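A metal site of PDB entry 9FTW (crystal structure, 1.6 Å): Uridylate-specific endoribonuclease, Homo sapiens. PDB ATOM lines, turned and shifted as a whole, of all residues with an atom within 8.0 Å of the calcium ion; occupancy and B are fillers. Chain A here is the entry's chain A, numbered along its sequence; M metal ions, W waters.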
ATOM      1  N   ALA A 200     -24.686  24.282   7.930  1.00  0.00           N
ATOM      2  CA  ALA A 200     -25.256  23.868   6.645  1.00  0.00           C
ATOM      3  C   ALA A 200     -24.970  22.356   6.382  1.00  0.00           C
ATOM      4  O   ALA A 200     -25.872  21.608   6.002  1.00  0.00           O
ATOM      5  CB  ALA A 200     -24.683  24.706   5.509  1.00  0.00           C
ATOM      6  N   ALA A 201     -23.730  21.918   6.638  1.00  0.00           N
ATOM      7  CA  ALA A 201     -23.362  20.506   6.432  1.00  0.00           C
ATOM      8  C   ALA A 201     -24.138  19.566   7.384  1.00  0.00           C
ATOM      9  O   ALA A 201     -24.618  18.508   6.967  1.00  0.00           O
ATOM     10  CB  ALA A 201     -21.870  20.329   6.620  1.00  0.00           C
ATOM     11  N   PHE A 202     -24.310  19.978   8.632  1.00  0.00           N
ATOM     12  CA  PHE A 202     -25.073  19.225   9.609  1.00  0.00           C
ATOM     13  C   PHE A 202     -26.539  19.114   9.174  1.00  0.00           C
ATOM     14  O   PHE A 202     -27.106  18.021   9.137  1.00  0.00           O
ATOM     15  CB  PHE A 202     -24.980  19.915  10.986  1.00  0.00           C
ATOM     16  CG  PHE A 202     -25.821  19.242  12.040  1.00  0.00           C
ATOM     17  CD1 PHE A 202     -25.459  18.010  12.558  1.00  0.00           C
ATOM     18  CD2 PHE A 202     -26.942  19.872  12.563  1.00  0.00           C
ATOM     19  CE1 PHE A 202     -26.219  17.391  13.551  1.00  0.00           C
ATOM     20  CE2 PHE A 202     -27.726  19.238  13.516  1.00  0.00           C
ATOM     21  CZ  PHE A 202     -27.365  17.991  14.001  1.00  0.00           C
ATOM     22  N   ILE A 203     -27.157  20.251   8.788  1.00  0.00           N
ATOM     23  CA  ILE A 203     -28.578  20.245   8.376  1.00  0.00           C
ATOM     24  C   ILE A 203     -28.806  19.369   7.138  1.00  0.00           C
ATOM     25  O   ILE A 203     -29.832  18.692   7.037  1.00  0.00           O
ATOM     26  CB  ILE A 203     -29.104  21.689   8.213  1.00  0.00           C
ATOM     27  CG1 ILE A 203     -29.170  22.391   9.607  1.00  0.00           C
ATOM     28  CG2 ILE A 203     -30.464  21.727   7.495  1.00  0.00           C
ATOM     29  CD1 ILE A 203     -29.217  23.925   9.525  1.00  0.00           C
ATOM     30  N   ASN A 204     -27.833  19.357   6.229  1.00  0.00           N
ATOM     31  CA  ASN A 204     -27.924  18.533   5.048  1.00  0.00           C
ATOM     32  C   ASN A 204     -28.021  17.032   5.386  1.00  0.00           C
ATOM     33  O   ASN A 204     -28.554  16.286   4.554  1.00  0.00           O
ATOM     34  CB  ASN A 204     -26.767  18.818   4.094  1.00  0.00           C
ATOM     35  CG  ASN A 204     -26.982  20.104   3.319  1.00  0.00           C
ATOM     36  OD1 ASN A 204     -28.116  20.623   3.234  1.00  0.00           O
ATOM     37  ND2 ASN A 204     -25.918  20.649   2.753  1.00  0.00           N
ATOM     38  N   LEU A 205     -27.523  16.594   6.551  1.00  0.00           N
ATOM     39  CA  LEU A 205     -27.616  15.178   6.959  1.00  0.00           C
ATOM     40  C   LEU A 205     -28.984  14.831   7.563  1.00  0.00           C
ATOM     41  O   LEU A 205     -29.396  13.652   7.530  1.00  0.00           O
ATOM     42  CB  LEU A 205     -26.528  14.876   8.009  1.00  0.00           C
ATOM     43  CG  LEU A 205     -25.081  14.894   7.500  1.00  0.00           C
ATOM     44  CD1 LEU A 205     -24.089  14.954   8.661  1.00  0.00           C
ATOM     45  CD2 LEU A 205     -24.752  13.627   6.658  1.00  0.00           C
ATOM     46  N   LEU A 206     -29.725  15.836   8.092  1.00  0.00           N
ATOM     47  CA  LEU A 206     -30.986  15.574   8.810  1.00  0.00           C
ATOM     48  C   LEU A 206     -32.177  15.110   7.947  1.00  0.00           C
ATOM     49  O   LEU A 206     -33.203  14.740   8.538  1.00  0.00           O
ATOM     50  CB  LEU A 206     -31.413  16.788   9.656  1.00  0.00           C
ATOM     51  CG  LEU A 206     -30.389  17.305  10.660  1.00  0.00           C
ATOM     52  CD1 LEU A 206     -30.908  18.612  11.340  1.00  0.00           C
ATOM     53  CD2 LEU A 206     -30.028  16.225  11.699  1.00  0.00           C
ATOM     54  N   ASN A 207     -32.075  15.091   6.619  1.00  0.00           N
ATOM     55  CA  ASN A 207     -33.133  14.562   5.746  1.00  0.00           C
ATOM     56  C   ASN A 207     -32.729  13.194   5.114  1.00  0.00           C
ATOM     57  O   ASN A 207     -33.426  12.729   4.198  1.00  0.00           O
ATOM     58  CB  ASN A 207     -33.505  15.559   4.630  1.00  0.00           C
ATOM     59  CG  ASN A 207     -32.455  15.760   3.562  1.00  0.00           C
ATOM     60  OD1 ASN A 207     -31.265  15.448   3.739  1.00  0.00           O
ATOM     61  ND2 ASN A 207     -32.887  16.314   2.417  1.00  0.00           N
ATOM     62  N   ASN A 208     -31.627  12.560   5.610  1.00  0.00           N
ATOM     63  CA  ASN A 208     -31.123  11.298   5.047  1.00  0.00           C
ATOM     64  C   ASN A 208     -31.718  10.019   5.682  1.00  0.00           C
ATOM     65  O   ASN A 208     -31.343   8.923   5.249  1.00  0.00           O
ATOM     66  CB  ASN A 208     -29.605  11.207   5.226  1.00  0.00           C
ATOM     67  CG  ASN A 208     -28.822  12.247   4.479  1.00  0.00           C
ATOM     68  OD1 ASN A 208     -29.409  13.136   3.827  1.00  0.00           O
ATOM     69  ND2 ASN A 208     -27.490  12.152   4.521  1.00  0.00           N
ATOM     70  N   TYR A 209     -32.601  10.132   6.684  1.00  0.00           N
ATOM     71  CA  TYR A 209     -33.020   8.964   7.461  1.00  0.00           C
ATOM     72  C   TYR A 209     -34.533   8.705   7.469  1.00  0.00           C
ATOM     73  O   TYR A 209     -35.318   9.565   7.075  1.00  0.00           O
ATOM     74  CB  TYR A 209     -32.533   9.216   8.929  1.00  0.00           C
ATOM     75  CG  TYR A 209     -31.021   9.342   9.018  1.00  0.00           C
ATOM     76  CD1 TYR A 209     -30.216   8.217   9.064  1.00  0.00           C
ATOM     77  CD2 TYR A 209     -30.404  10.591   8.975  1.00  0.00           C
ATOM     78  CE1 TYR A 209     -28.841   8.324   9.093  1.00  0.00           C
ATOM     79  CE2 TYR A 209     -29.030  10.712   8.938  1.00  0.00           C
ATOM     80  CZ  TYR A 209     -28.239   9.571   9.065  1.00  0.00           C
ATOM     81  OH  TYR A 209     -26.869   9.638   9.026  1.00  0.00           O
ATOM     82  N   SER A 220     -27.396   7.385  -0.722  1.00  0.00           N
ATOM     83  CA  SER A 220     -26.955   7.610  -2.094  1.00  0.00           C
ATOM     84  C   SER A 220     -25.469   8.070  -2.032  1.00  0.00           C
ATOM     85  O   SER A 220     -24.978   8.428  -0.965  1.00  0.00           O
ATOM     86  CB  SER A 220     -27.814   8.700  -2.738  1.00  0.00           C
ATOM     87  OG  SER A 220     -27.613   9.917  -2.033  1.00  0.00           O
ATOM     88  N   GLN A 222     -24.455  10.929  -2.990  1.00  0.00           N
ATOM     89  CA  GLN A 222     -24.518  12.324  -2.526  1.00  0.00           C
ATOM     90  C   GLN A 222     -24.704  12.373  -1.002  1.00  0.00           C
ATOM     91  O   GLN A 222     -24.112  13.215  -0.340  1.00  0.00           O
ATOM     92  CB  GLN A 222     -25.641  13.072  -3.265  1.00  0.00           C
ATOM     93  CG  GLN A 222     -25.507  13.000  -4.818  1.00  0.00           C
ATOM     94  CD  GLN A 222     -26.443  11.951  -5.418  1.00  0.00           C
ATOM     95  OE1 GLN A 222     -26.257  10.729  -5.245  1.00  0.00           O
ATOM     96  NE2 GLN A 222     -27.484  12.416  -6.138  1.00  0.00           N
ATOM     97  N   GLU A 223     -25.443  11.414  -0.429  1.00  0.00           N
ATOM     98  CA  GLU A 223     -25.607  11.333   1.026  1.00  0.00           C
ATOM     99  C   GLU A 223     -24.303  10.908   1.746  1.00  0.00           C
ATOM    100  O   GLU A 223     -23.987  11.473   2.800  1.00  0.00           O
ATOM    101  CB  GLU A 223     -26.792  10.440   1.367  1.00  0.00           C
ATOM    102  CG  GLU A 223     -28.111  11.136   1.080  1.00  0.00           C
ATOM    103  CD  GLU A 223     -29.360  10.304   1.114  1.00  0.00           C
ATOM    104  OE1 GLU A 223     -29.270   9.057   1.054  1.00  0.00           O
ATOM    105  OE2 GLU A 223     -30.458  10.904   1.197  1.00  0.00           O
ATOM    106  N   LEU A 224     -23.496  10.009   1.160  1.00  0.00           N
ATOM    107  CA  LEU A 224     -22.185   9.667   1.759  1.00  0.00           C
ATOM    108  C   LEU A 224     -21.237  10.874   1.591  1.00  0.00           C
ATOM    109  O   LEU A 224     -20.477  11.163   2.511  1.00  0.00           O
ATOM    110  CB  LEU A 224     -21.564   8.425   1.102  1.00  0.00           C
ATOM    111  CG  LEU A 224     -22.341   7.101   1.276  1.00  0.00           C
ATOM    112  CD1 LEU A 224     -21.768   6.030   0.351  1.00  0.00           C
ATOM    113  CD2 LEU A 224     -22.298   6.606   2.725  1.00  0.00           C
ATOM    114  N   GLU A 226     -22.239  13.903   1.803  1.00  0.00           N
ATOM    115  CA  GLU A 226     -22.665  14.801   2.897  1.00  0.00           C
ATOM    116  C   GLU A 226     -21.975  14.445   4.220  1.00  0.00           C
ATOM    117  O   GLU A 226     -21.647  15.353   5.008  1.00  0.00           O
ATOM    118  CB  GLU A 226     -24.197  14.733   3.110  1.00  0.00           C
ATOM    119  CG  GLU A 226     -24.974  15.449   2.017  1.00  0.00           C
ATOM    120  CD  GLU A 226     -26.484  15.334   2.119  1.00  0.00           C
ATOM    121  OE1 GLU A 226     -26.960  14.380   2.768  1.00  0.00           O
ATOM    122  OE2 GLU A 226     -27.180  16.223   1.574  1.00  0.00           O
ATOM    123  N   GLN A 227     -21.731  13.160   4.474  1.00  0.00           N
ATOM    124  CA  GLN A 227     -21.055  12.746   5.718  1.00  0.00           C
ATOM    125  C   GLN A 227     -19.600  13.243   5.693  1.00  0.00           C
ATOM    126  O   GLN A 227     -19.120  13.874   6.651  1.00  0.00           O
ATOM    127  CB  GLN A 227     -21.085  11.216   5.805  1.00  0.00           C
ATOM    128  CG  GLN A 227     -22.472  10.625   5.976  1.00  0.00           C
ATOM    129  CD  GLN A 227     -22.406   9.099   6.013  1.00  0.00           C
ATOM    130  OE1 GLN A 227     -21.332   8.481   5.962  1.00  0.00           O
ATOM    131  NE2 GLN A 227     -23.564   8.451   6.082  1.00  0.00           N
HETATM  132 CA    CA M   1     -29.224  15.179   2.682  1.00  0.00          CA
HETATM  133  O   HOH W   1     -30.077  17.220   1.592  1.00  0.00           O
HETATM  134  O   HOH W   2     -30.185  14.003   0.914  1.00  0.00           O
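ND2 of Asn 204 lies close to O of Ala 200, 3.4 Å away.
Of the 16 residues printed, 4 come within 4 Å of the calcium ion.
The calcium ion is bound by the backbone carbonyl oxygen (O) of Asn 204, the side-chain amide oxygen (OD1) of Asn 207, water W2, the side-chain amide oxygen (OD1) of Asn 208, the side-chain carboxylate (OE1) of Glu 226, water W1 and the side-chain carboxylate (OE2) of Glu 226. The calcium ion has seven donor atoms within binding distance.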
